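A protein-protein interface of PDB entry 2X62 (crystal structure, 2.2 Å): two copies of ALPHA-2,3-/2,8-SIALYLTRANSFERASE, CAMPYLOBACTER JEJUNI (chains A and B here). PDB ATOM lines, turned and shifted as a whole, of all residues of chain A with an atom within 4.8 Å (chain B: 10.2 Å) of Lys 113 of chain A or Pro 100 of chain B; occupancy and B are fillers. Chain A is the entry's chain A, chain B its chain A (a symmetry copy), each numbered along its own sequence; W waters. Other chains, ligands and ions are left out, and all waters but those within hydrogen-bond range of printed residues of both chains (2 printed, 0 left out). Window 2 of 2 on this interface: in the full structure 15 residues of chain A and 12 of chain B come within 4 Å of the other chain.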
ATOM      1  N   LYS A 110     -11.461  -4.114  18.013  1.00  0.00           N
ATOM      2  CA  LYS A 110     -12.239  -3.596  16.896  1.00  0.00           C
ATOM      3  C   LYS A 110     -13.746  -3.623  17.162  1.00  0.00           C
ATOM      4  O   LYS A 110     -14.503  -2.957  16.474  1.00  0.00           O
ATOM      5  CB  LYS A 110     -11.907  -4.341  15.603  1.00  0.00           C
ATOM      6  CG  LYS A 110     -12.586  -5.675  15.441  1.00  0.00           C
ATOM      7  CD  LYS A 110     -12.070  -6.366  14.185  1.00  0.00           C
ATOM      8  CE  LYS A 110     -12.417  -7.842  14.186  1.00  0.00           C
ATOM      9  NZ  LYS A 110     -11.746  -8.539  13.074  1.00  0.00           N
ATOM     10  N   GLN A 111     -14.172  -4.341  18.198  1.00  0.00           N
ATOM     11  CA  GLN A 111     -15.588  -4.346  18.570  1.00  0.00           C
ATOM     12  C   GLN A 111     -16.010  -2.998  19.166  1.00  0.00           C
ATOM     13  O   GLN A 111     -17.179  -2.732  19.278  1.00  0.00           O
ATOM     14  CB  GLN A 111     -15.883  -5.483  19.562  1.00  0.00           C
ATOM     15  CG  GLN A 111     -15.574  -6.854  18.967  1.00  0.00           C
ATOM     16  CD  GLN A 111     -15.973  -8.001  19.871  1.00  0.00           C
ATOM     17  OE1 GLN A 111     -15.290  -9.028  19.942  1.00  0.00           O
ATOM     18  NE2 GLN A 111     -17.078  -7.846  20.549  1.00  0.00           N
ATOM     19  N   LEU A 112     -15.045  -2.172  19.575  1.00  0.00           N
ATOM     20  CA  LEU A 112     -15.328  -0.817  20.074  1.00  0.00           C
ATOM     21  C   LEU A 112     -15.082   0.125  18.926  1.00  0.00           C
ATOM     22  O   LEU A 112     -14.002   0.725  18.801  1.00  0.00           O
ATOM     23  CB  LEU A 112     -14.404  -0.434  21.219  1.00  0.00           C
ATOM     24  CG  LEU A 112     -14.326  -1.354  22.433  1.00  0.00           C
ATOM     25  CD1 LEU A 112     -13.542  -0.694  23.515  1.00  0.00           C
ATOM     26  CD2 LEU A 112     -15.709  -1.651  22.917  1.00  0.00           C
ATOM     27  N   LYS A 113     -16.079   0.249  18.061  1.00  0.00           N
ATOM     28  CA  LYS A 113     -15.851   0.891  16.802  1.00  0.00           C
ATOM     29  C   LYS A 113     -15.464   2.364  16.963  1.00  0.00           C
ATOM     30  O   LYS A 113     -14.551   2.841  16.324  1.00  0.00           O
ATOM     31  CB  LYS A 113     -17.099   0.735  15.950  1.00  0.00           C
ATOM     32  CG  LYS A 113     -16.982   1.312  14.599  1.00  0.00           C
ATOM     33  CD  LYS A 113     -18.303   1.881  14.168  1.00  0.00           C
ATOM     34  CE  LYS A 113     -19.376   0.826  14.079  1.00  0.00           C
ATOM     35  NZ  LYS A 113     -20.627   1.528  13.655  1.00  0.00           N
ATOM     36  N   ASP A 114     -16.147   3.091  17.829  1.00  0.00           N
ATOM     37  CA  ASP A 114     -15.842   4.502  18.027  1.00  0.00           C
ATOM     38  C   ASP A 114     -14.403   4.677  18.540  1.00  0.00           C
ATOM     39  O   ASP A 114     -13.696   5.605  18.157  1.00  0.00           O
ATOM     40  CB  ASP A 114     -16.822   5.117  19.016  1.00  0.00           C
ATOM     41  CG  ASP A 114     -18.182   5.348  18.413  1.00  0.00           C
ATOM     42  OD1 ASP A 114     -18.359   5.014  17.226  1.00  0.00           O
ATOM     43  OD2 ASP A 114     -19.067   5.894  19.112  1.00  0.00           O
ATOM     44  N   PHE A 115     -13.970   3.764  19.393  1.00  0.00           N
ATOM     45  CA  PHE A 115     -12.618   3.831  19.896  1.00  0.00           C
ATOM     46  C   PHE A 115     -11.570   3.401  18.881  1.00  0.00           C
ATOM     47  O   PHE A 115     -10.495   3.995  18.823  1.00  0.00           O
ATOM     48  CB  PHE A 115     -12.445   3.028  21.174  1.00  0.00           C
ATOM     49  CG  PHE A 115     -11.151   3.318  21.875  1.00  0.00           C
ATOM     50  CD1 PHE A 115     -10.836   4.610  22.261  1.00  0.00           C
ATOM     51  CD2 PHE A 115     -10.243   2.316  22.137  1.00  0.00           C
ATOM     52  CE1 PHE A 115      -9.672   4.896  22.904  1.00  0.00           C
ATOM     53  CE2 PHE A 115      -9.073   2.604  22.768  1.00  0.00           C
ATOM     54  CZ  PHE A 115      -8.783   3.911  23.151  1.00  0.00           C
ATOM     55  N   ASN A 116     -11.850   2.366  18.103  1.00  0.00           N
ATOM     56  CA  ASN A 116     -10.950   1.990  17.018  1.00  0.00           C
ATOM     57  C   ASN A 116     -10.760   3.205  16.088  1.00  0.00           C
ATOM     58  O   ASN A 116      -9.647   3.561  15.745  1.00  0.00           O
ATOM     59  CB  ASN A 116     -11.510   0.801  16.268  1.00  0.00           C
ATOM     60  CG  ASN A 116     -10.485   0.098  15.395  1.00  0.00           C
ATOM     61  OD1 ASN A 116      -9.294   0.373  15.432  1.00  0.00           O
ATOM     62  ND2 ASN A 116     -10.965  -0.821  14.593  1.00  0.00           N
ATOM     63  N   ALA A 117     -11.857   3.866  15.734  1.00  0.00           N
ATOM     64  CA  ALA A 117     -11.785   5.083  14.943  1.00  0.00           C
ATOM     65  C   ALA A 117     -10.974   6.178  15.642  1.00  0.00           C
ATOM     66  O   ALA A 117     -10.108   6.800  15.031  1.00  0.00           O
ATOM     67  CB  ALA A 117     -13.161   5.572  14.600  1.00  0.00           C
ATOM     68  N   LYS A 120      -7.261   5.145  15.589  1.00  0.00           N
ATOM     69  CA  LYS A 120      -6.685   5.149  14.254  1.00  0.00           C
ATOM     70  C   LYS A 120      -6.458   6.574  13.779  1.00  0.00           C
ATOM     71  O   LYS A 120      -5.411   6.910  13.235  1.00  0.00           O
ATOM     72  CB  LYS A 120      -7.625   4.405  13.299  1.00  0.00           C
ATOM     73  CG  LYS A 120      -7.704   2.883  13.520  1.00  0.00           C
ATOM     74  CD  LYS A 120      -6.395   2.213  13.164  1.00  0.00           C
ATOM     75  CE  LYS A 120      -6.301   0.841  13.819  1.00  0.00           C
ATOM     76  NZ  LYS A 120      -7.334  -0.128  13.337  1.00  0.00           N
ATOM     77  N   TYR A 204     -18.433   4.451  26.627  1.00  0.00           N
ATOM     78  CA  TYR A 204     -18.950   3.124  26.918  1.00  0.00           C
ATOM     79  C   TYR A 204     -19.562   3.006  28.329  1.00  0.00           C
ATOM     80  O   TYR A 204     -19.909   1.920  28.770  1.00  0.00           O
ATOM     81  CB  TYR A 204     -17.884   2.043  26.640  1.00  0.00           C
ATOM     82  CG  TYR A 204     -17.443   2.072  25.190  1.00  0.00           C
ATOM     83  CD1 TYR A 204     -18.266   1.592  24.193  1.00  0.00           C
ATOM     84  CD2 TYR A 204     -16.242   2.664  24.814  1.00  0.00           C
ATOM     85  CE1 TYR A 204     -17.904   1.684  22.885  1.00  0.00           C
ATOM     86  CE2 TYR A 204     -15.862   2.745  23.498  1.00  0.00           C
ATOM     87  CZ  TYR A 204     -16.685   2.265  22.548  1.00  0.00           C
ATOM     88  OH  TYR A 204     -16.324   2.349  21.242  1.00  0.00           O
ATOM     89  N   PHE B  55      -9.619  10.090  -0.683  1.00  0.00           N
ATOM     90  CA  PHE B  55     -10.336   9.730   0.538  1.00  0.00           C
ATOM     91  C   PHE B  55      -9.509  10.000   1.783  1.00  0.00           C
ATOM     92  O   PHE B  55     -10.039  10.480   2.784  1.00  0.00           O
ATOM     93  CB  PHE B  55     -10.797   8.258   0.542  1.00  0.00           C
ATOM     94  CG  PHE B  55     -11.706   7.945   1.689  1.00  0.00           C
ATOM     95  CD1 PHE B  55     -13.058   8.104   1.565  1.00  0.00           C
ATOM     96  CD2 PHE B  55     -11.188   7.548   2.911  1.00  0.00           C
ATOM     97  CE1 PHE B  55     -13.905   7.838   2.644  1.00  0.00           C
ATOM     98  CE2 PHE B  55     -12.011   7.299   3.988  1.00  0.00           C
ATOM     99  CZ  PHE B  55     -13.379   7.456   3.859  1.00  0.00           C
ATOM    100  N   TYR B  59     -11.051  12.484   4.469  1.00  0.00           N
ATOM    101  CA  TYR B  59     -11.389  11.971   5.809  1.00  0.00           C
ATOM    102  C   TYR B  59     -10.806  12.869   6.922  1.00  0.00           C
ATOM    103  O   TYR B  59     -11.490  13.216   7.894  1.00  0.00           O
ATOM    104  CB  TYR B  59     -10.899  10.517   5.965  1.00  0.00           C
ATOM    105  CG  TYR B  59     -11.315   9.872   7.257  1.00  0.00           C
ATOM    106  CD1 TYR B  59     -12.557   9.256   7.390  1.00  0.00           C
ATOM    107  CD2 TYR B  59     -10.471   9.865   8.346  1.00  0.00           C
ATOM    108  CE1 TYR B  59     -12.945   8.668   8.595  1.00  0.00           C
ATOM    109  CE2 TYR B  59     -10.842   9.275   9.532  1.00  0.00           C
ATOM    110  CZ  TYR B  59     -12.075   8.688   9.661  1.00  0.00           C
ATOM    111  OH  TYR B  59     -12.407   8.112  10.870  1.00  0.00           O
ATOM    112  N   LYS B  63     -12.903  15.337   9.642  1.00  0.00           N
ATOM    113  CA  LYS B  63     -12.719  15.347  11.082  1.00  0.00           C
ATOM    114  C   LYS B  63     -12.519  16.767  11.571  1.00  0.00           C
ATOM    115  O   LYS B  63     -12.977  17.097  12.644  1.00  0.00           O
ATOM    116  CB  LYS B  63     -11.547  14.474  11.515  1.00  0.00           C
ATOM    117  CG  LYS B  63     -11.772  13.016  11.196  1.00  0.00           C
ATOM    118  CD  LYS B  63     -12.587  12.341  12.287  1.00  0.00           C
ATOM    119  CE  LYS B  63     -13.165  11.021  11.829  1.00  0.00           C
ATOM    120  NZ  LYS B  63     -13.865  10.341  12.970  1.00  0.00           N
ATOM    121  N   GLU B  74     -23.747  11.489  10.109  1.00  0.00           N
ATOM    122  CA  GLU B  74     -23.821  10.191  10.740  1.00  0.00           C
ATOM    123  C   GLU B  74     -22.971   9.142  10.002  1.00  0.00           C
ATOM    124  O   GLU B  74     -22.347   8.316  10.633  1.00  0.00           O
ATOM    125  CB  GLU B  74     -25.261   9.736  10.801  1.00  0.00           C
ATOM    126  CG  GLU B  74     -25.411   8.405  11.457  1.00  0.00           C
ATOM    127  CD  GLU B  74     -26.846   7.921  11.467  1.00  0.00           C
ATOM    128  OE1 GLU B  74     -27.780   8.762  11.560  1.00  0.00           O
ATOM    129  OE2 GLU B  74     -27.015   6.688  11.375  1.00  0.00           O
ATOM    130  N   LEU B  75     -22.927   9.185   8.673  1.00  0.00           N
ATOM    131  CA  LEU B  75     -22.249   8.130   7.922  1.00  0.00           C
ATOM    132  C   LEU B  75     -21.169   8.712   7.043  1.00  0.00           C
ATOM    133  O   LEU B  75     -21.288   9.848   6.550  1.00  0.00           O
ATOM    134  CB  LEU B  75     -23.235   7.343   7.047  1.00  0.00           C
ATOM    135  CG  LEU B  75     -24.367   6.633   7.761  1.00  0.00           C
ATOM    136  CD1 LEU B  75     -25.421   6.265   6.751  1.00  0.00           C
ATOM    137  CD2 LEU B  75     -23.903   5.395   8.525  1.00  0.00           C
ATOM    138  N   ILE B  76     -20.100   7.948   6.867  1.00  0.00           N
ATOM    139  CA  ILE B  76     -19.030   8.332   5.974  1.00  0.00           C
ATOM    140  C   ILE B  76     -18.804   7.210   4.958  1.00  0.00           C
ATOM    141  O   ILE B  76     -18.472   6.084   5.353  1.00  0.00           O
ATOM    142  CB  ILE B  76     -17.747   8.589   6.753  1.00  0.00           C
ATOM    143  CG1 ILE B  76     -17.998   9.674   7.804  1.00  0.00           C
ATOM    144  CG2 ILE B  76     -16.642   9.011   5.812  1.00  0.00           C
ATOM    145  CD1 ILE B  76     -16.946   9.704   8.918  1.00  0.00           C
ATOM    146  N   MET B  77     -18.961   7.538   3.663  1.00  0.00           N
ATOM    147  CA  MET B  77     -18.883   6.581   2.587  1.00  0.00           C
ATOM    148  C   MET B  77     -17.765   6.883   1.593  1.00  0.00           C
ATOM    149  O   MET B  77     -17.594   8.029   1.191  1.00  0.00           O
ATOM    150  CB  MET B  77     -20.177   6.565   1.789  1.00  0.00           C
ATOM    151  CG  MET B  77     -21.430   6.286   2.544  1.00  0.00           C
ATOM    152  SD  MET B  77     -21.924   4.571   2.516  1.00  0.00           S
ATOM    153  CE  MET B  77     -23.442   4.588   3.467  1.00  0.00           C
ATOM    154  N   THR B  94      -8.010  -2.940   3.148  1.00  0.00           N
ATOM    155  CA  THR B  94      -7.696  -2.547   4.525  1.00  0.00           C
ATOM    156  C   THR B  94      -8.569  -1.429   5.057  1.00  0.00           C
ATOM    157  O   THR B  94      -8.373  -0.965   6.192  1.00  0.00           O
ATOM    158  CB  THR B  94      -6.271  -2.043   4.609  1.00  0.00           C
ATOM    159  OG1 THR B  94      -6.115  -0.889   3.763  1.00  0.00           O
ATOM    160  CG2 THR B  94      -5.308  -3.138   4.201  1.00  0.00           C
ATOM    161  N   PHE B  95      -9.532  -1.015   4.241  1.00  0.00           N
ATOM    162  CA  PHE B  95     -10.349   0.173   4.514  1.00  0.00           C
ATOM    163  C   PHE B  95     -10.895   0.288   5.934  1.00  0.00           C
ATOM    164  O   PHE B  95     -10.726   1.318   6.595  1.00  0.00           O
ATOM    165  CB  PHE B  95     -11.531   0.208   3.558  1.00  0.00           C
ATOM    166  CG  PHE B  95     -12.338   1.466   3.650  1.00  0.00           C
ATOM    167  CD1 PHE B  95     -11.963   2.593   2.956  1.00  0.00           C
ATOM    168  CD2 PHE B  95     -13.500   1.513   4.434  1.00  0.00           C
ATOM    169  CE1 PHE B  95     -12.700   3.750   3.061  1.00  0.00           C
ATOM    170  CE2 PHE B  95     -14.228   2.648   4.537  1.00  0.00           C
ATOM    171  CZ  PHE B  95     -13.833   3.791   3.840  1.00  0.00           C
ATOM    172  N   TYR B  96     -11.578  -0.760   6.385  1.00  0.00           N
ATOM    173  CA  TYR B  96     -12.269  -0.734   7.665  1.00  0.00           C
ATOM    174  C   TYR B  96     -11.314  -0.675   8.863  1.00  0.00           C
ATOM    175  O   TYR B  96     -11.725  -0.367   9.977  1.00  0.00           O
ATOM    176  CB  TYR B  96     -13.199  -1.942   7.771  1.00  0.00           C
ATOM    177  CG  TYR B  96     -14.479  -1.732   6.995  1.00  0.00           C
ATOM    178  CD1 TYR B  96     -14.717  -2.409   5.802  1.00  0.00           C
ATOM    179  CD2 TYR B  96     -15.431  -0.836   7.445  1.00  0.00           C
ATOM    180  CE1 TYR B  96     -15.883  -2.206   5.082  1.00  0.00           C
ATOM    181  CE2 TYR B  96     -16.601  -0.607   6.722  1.00  0.00           C
ATOM    182  CZ  TYR B  96     -16.819  -1.283   5.550  1.00  0.00           C
ATOM    183  OH  TYR B  96     -17.979  -1.059   4.859  1.00  0.00           O
ATOM    184  N   ASP B  97     -10.047  -0.964   8.629  1.00  0.00           N
ATOM    185  CA  ASP B  97      -9.064  -0.951   9.677  1.00  0.00           C
ATOM    186  C   ASP B  97      -8.357   0.377   9.710  1.00  0.00           C
ATOM    187  O   ASP B  97      -7.816   0.741  10.747  1.00  0.00           O
ATOM    188  CB  ASP B  97      -8.055  -2.063   9.459  1.00  0.00           C
ATOM    189  CG  ASP B  97      -8.646  -3.448   9.712  1.00  0.00           C
ATOM    190  OD1 ASP B  97      -9.496  -3.624  10.612  1.00  0.00           O
ATOM    191  OD2 ASP B  97      -8.255  -4.358   8.993  1.00  0.00           O
ATOM    192  N   TYR B  98      -8.366   1.107   8.586  1.00  0.00           N
ATOM    193  CA  TYR B  98      -7.822   2.465   8.561  1.00  0.00           C
ATOM    194  C   TYR B  98      -8.873   3.513   8.908  1.00  0.00           C
ATOM    195  O   TYR B  98      -8.525   4.584   9.438  1.00  0.00           O
ATOM    196  CB  TYR B  98      -7.144   2.785   7.216  1.00  0.00           C
ATOM    197  CG  TYR B  98      -5.781   2.149   7.143  1.00  0.00           C
ATOM    198  CD1 TYR B  98      -5.640   0.801   6.842  1.00  0.00           C
ATOM    199  CD2 TYR B  98      -4.655   2.867   7.490  1.00  0.00           C
ATOM    200  CE1 TYR B  98      -4.393   0.198   6.832  1.00  0.00           C
ATOM    201  CE2 TYR B  98      -3.421   2.298   7.483  1.00  0.00           C
ATOM    202  CZ  TYR B  98      -3.289   0.966   7.145  1.00  0.00           C
ATOM    203  OH  TYR B  98      -2.057   0.408   7.181  1.00  0.00           O
ATOM    204  N   PHE B  99     -10.145   3.192   8.615  1.00  0.00           N
ATOM    205  CA  PHE B  99     -11.247   4.117   8.816  1.00  0.00           C
ATOM    206  C   PHE B  99     -12.429   3.432   9.485  1.00  0.00           C
ATOM    207  O   PHE B  99     -13.447   3.165   8.867  1.00  0.00           O
ATOM    208  CB  PHE B  99     -11.657   4.729   7.485  1.00  0.00           C
ATOM    209  CG  PHE B  99     -10.498   5.279   6.705  1.00  0.00           C
ATOM    210  CD1 PHE B  99      -9.993   4.593   5.631  1.00  0.00           C
ATOM    211  CD2 PHE B  99      -9.918   6.478   7.064  1.00  0.00           C
ATOM    212  CE1 PHE B  99      -8.909   5.097   4.933  1.00  0.00           C
ATOM    213  CE2 PHE B  99      -8.878   6.996   6.367  1.00  0.00           C
ATOM    214  CZ  PHE B  99      -8.357   6.297   5.302  1.00  0.00           C
ATOM    215  N   PRO B 100     -12.292   3.123  10.770  1.00  0.00           N
ATOM    216  CA  PRO B 100     -13.256   2.144  11.264  1.00  0.00           C
ATOM    217  C   PRO B 100     -14.682   2.667  11.375  1.00  0.00           C
ATOM    218  O   PRO B 100     -15.592   1.865  11.459  1.00  0.00           O
ATOM    219  CB  PRO B 100     -12.707   1.789  12.636  1.00  0.00           C
ATOM    220  CG  PRO B 100     -11.216   2.059  12.520  1.00  0.00           C
ATOM    221  CD  PRO B 100     -11.145   3.279  11.662  1.00  0.00           C
ATOM    222  N   ASP B 101     -14.873   3.992  11.388  1.00  0.00           N
ATOM    223  CA  ASP B 101     -16.228   4.567  11.439  1.00  0.00           C
ATOM    224  C   ASP B 101     -16.799   4.900  10.065  1.00  0.00           C
ATOM    225  O   ASP B 101     -17.865   5.517   9.953  1.00  0.00           O
ATOM    226  CB  ASP B 101     -16.280   5.816  12.336  1.00  0.00           C
ATOM    227  CG  ASP B 101     -15.253   6.905  11.945  1.00  0.00           C
ATOM    228  OD1 ASP B 101     -14.454   6.742  11.009  1.00  0.00           O
ATOM    229  OD2 ASP B 101     -15.244   7.958  12.604  1.00  0.00           O
ATOM    230  N   ALA B 102     -16.114   4.467   9.014  1.00  0.00           N
ATOM    231  CA  ALA B 102     -16.575   4.718   7.664  1.00  0.00           C
ATOM    232  C   ALA B 102     -17.082   3.458   7.012  1.00  0.00           C
ATOM    233  O   ALA B 102     -16.989   2.355   7.571  1.00  0.00           O
ATOM    234  CB  ALA B 102     -15.448   5.287   6.863  1.00  0.00           C
ATOM    235  N   HIS B 103     -17.600   3.621   5.805  1.00  0.00           N
ATOM    236  CA  HIS B 103     -18.107   2.506   5.010  1.00  0.00           C
ATOM    237  C   HIS B 103     -17.604   2.573   3.582  1.00  0.00           C
ATOM    238  O   HIS B 103     -17.436   3.638   3.003  1.00  0.00           O
ATOM    239  CB  HIS B 103     -19.635   2.536   4.989  1.00  0.00           C
ATOM    240  CG  HIS B 103     -20.260   2.035   6.245  1.00  0.00           C
ATOM    241  ND1 HIS B 103     -20.701   2.871   7.239  1.00  0.00           N
ATOM    242  CD2 HIS B 103     -20.509   0.774   6.672  1.00  0.00           C
ATOM    243  CE1 HIS B 103     -21.209   2.151   8.221  1.00  0.00           C
ATOM    244  NE2 HIS B 103     -21.085   0.876   7.907  1.00  0.00           N
ATOM    245  N   LEU B 104     -17.334   1.424   3.012  1.00  0.00           N
ATOM    246  CA  LEU B 104     -17.201   1.321   1.565  1.00  0.00           C
ATOM    247  C   LEU B 104     -18.610   1.335   0.975  1.00  0.00           C
ATOM    248  O   LEU B 104     -19.428   0.502   1.315  1.00  0.00           O
ATOM    249  CB  LEU B 104     -16.532   0.015   1.210  1.00  0.00           C
ATOM    250  CG  LEU B 104     -15.078  -0.174   1.631  1.00  0.00           C
ATOM    251  CD1 LEU B 104     -14.641  -1.590   1.435  1.00  0.00           C
ATOM    252  CD2 LEU B 104     -14.194   0.758   0.828  1.00  0.00           C
ATOM    253  N   ASP B 107     -20.416  -1.815  -0.470  1.00  0.00           N
ATOM    254  CA  ASP B 107     -21.179  -2.711   0.418  1.00  0.00           C
ATOM    255  C   ASP B 107     -22.693  -2.535   0.226  1.00  0.00           C
ATOM    256  O   ASP B 107     -23.514  -3.483   0.385  1.00  0.00           O
ATOM    257  CB  ASP B 107     -20.844  -2.409   1.874  1.00  0.00           C
ATOM    258  CG  ASP B 107     -19.526  -3.009   2.326  1.00  0.00           C
ATOM    259  OD1 ASP B 107     -18.856  -3.688   1.527  1.00  0.00           O
ATOM    260  OD2 ASP B 107     -19.149  -2.787   3.501  1.00  0.00           O
ATOM    261  N   PHE B 108     -23.070  -1.304  -0.095  1.00  0.00           N
ATOM    262  CA  PHE B 108     -24.470  -0.959  -0.357  1.00  0.00           C
ATOM    263  C   PHE B 108     -24.819  -0.982  -1.849  1.00  0.00           C
ATOM    264  O   PHE B 108     -25.823  -1.535  -2.240  1.00  0.00           O
ATOM    265  CB  PHE B 108     -24.761   0.399   0.274  1.00  0.00           C
ATOM    266  CG  PHE B 108     -24.452   0.428   1.745  1.00  0.00           C
ATOM    267  CD1 PHE B 108     -23.276   0.958   2.210  1.00  0.00           C
ATOM    268  CD2 PHE B 108     -25.307  -0.170   2.658  1.00  0.00           C
ATOM    269  CE1 PHE B 108     -22.986   0.955   3.571  1.00  0.00           C
ATOM    270  CE2 PHE B 108     -25.015  -0.175   4.002  1.00  0.00           C
ATOM    271  CZ  PHE B 108     -23.860   0.391   4.452  1.00  0.00           C
ATOM    272  N   PHE B 254       0.219   5.622   5.130  1.00  0.00           N
ATOM    273  CA  PHE B 254      -0.905   5.229   4.303  1.00  0.00           C
ATOM    274  C   PHE B 254      -0.455   4.846   2.894  1.00  0.00           C
ATOM    275  O   PHE B 254      -1.271   4.530   2.037  1.00  0.00           O
ATOM    276  CB  PHE B 254      -1.899   6.378   4.226  1.00  0.00           C
ATOM    277  CG  PHE B 254      -3.256   5.963   3.775  1.00  0.00           C
ATOM    278  CD1 PHE B 254      -3.744   6.353   2.538  1.00  0.00           C
ATOM    279  CD2 PHE B 254      -4.040   5.146   4.574  1.00  0.00           C
ATOM    280  CE1 PHE B 254      -5.001   5.946   2.112  1.00  0.00           C
ATOM    281  CE2 PHE B 254      -5.273   4.737   4.166  1.00  0.00           C
ATOM    282  CZ  PHE B 254      -5.774   5.151   2.937  1.00  0.00           C
HETATM  283  O   HOH W   1     -12.234   9.494  15.251  1.00  0.00           O
HETATM  284  O   HOH W   2     -10.377   6.630  12.259  1.00  0.00           O
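Water W2 bridges the backbone carbonyl oxygen (O) of Ala 117 of chain A and the side-chain hydroxyl (OH) of Tyr 59 of chain B.
Water W1 bridges the side-chain amino group of Lys 63 of chain B (2.9 Å) and the backbone carbonyl oxygen of Ala 117 of chain A (3.4 Å).
No position is printed for both chains.
Of the 7 pairs that touch across the chains among the printed residues, none has its exchanged pair printed and touching as well.
The backbone carbonyl oxygen of Asp 97 of chain B lies within hydrogen-bond range of the side-chain amino group of Lys 120 of chain A, 2.8 Å away.
Lys 113 of chain A touches just one residue of chain B: Pro 100.
Pro 100 of chain B touches just these residues of chain A: Lys 113 (3.5 Å), Asn 116 (3.6 Å), Ala 117 (3.7 Å) and Lys 120 (3.7 Å).
No residue of chain B comes within 4 Å of Leu 112 of chain A.
Asp 114 of chain A touches none of the printed residues of chain B.
Asn 116 of chain A touches one residue of chain B.
Ala 117 of chain A touches just these residues of chain B: Pro 100 (3.7 Å) and Asp 101 (3.6 Å).
Of the printed residues of chain A, Asp 101 of chain B touches Ala 117 (3.6 Å).
Of the printed residues of chain A, Asp 97 of chain B touches Lys 120.
Of the printed residues of chain A, Tyr 98 of chain B touches Lys 120.
Printed residues of chain B within 4 Å of Lys 120 of chain A: Asp 97, Tyr 98 and Pro 100.
Ile 76 of chain B touches none of the printed residues of chain A.
Leu 104 of chain B touches none of the printed residues of chain A.
The nearest printed residue of chain A that does not touch Pro 100 of chain B is Lys 110 of chain A (6.4 Å).
NZ of Lys 120 of chain A lies within hydrogen-bond range of OD1 of Asn 116 of chain A (2.9 Å).
The side-chain carboxylate (OD1) of Asp 101 of chain B lies within hydrogen-bond range of the side-chain hydroxyl (OH) of Tyr 59 of chain B (2.5 Å).
NZ of Lys 63 of chain B lies within salt-bridge range of OD2 of Asp 101 of chain B, at 2.8 Å.
Of the 10 printed residues of chain A, 4 touch a printed residue of chain B.
Hydrophobic or aromatic side chains of chain A that line the printed part of chain B: Ala 117.
Among the printed residues, 7 pairs touch across the chains.
Pro 100 of chain B touches Lys 113 of chain A (O to CG, 3.5 Å).
Pro 100 of chain B touches Asn 116 of chain A.
Pro 100 of chain B touches Ala 117 of chain A (CG to N, 3.7 Å).
Asp 101 of chain B touches Ala 117 of chain A (CG to CB, 3.6 Å).
O of Tyr 98 of chain B touches CB of Lys 120 of chain A, at 3.97 Å.
CG of Pro 100 of chain B touches CG of Lys 120 of chain A (3.7 Å).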
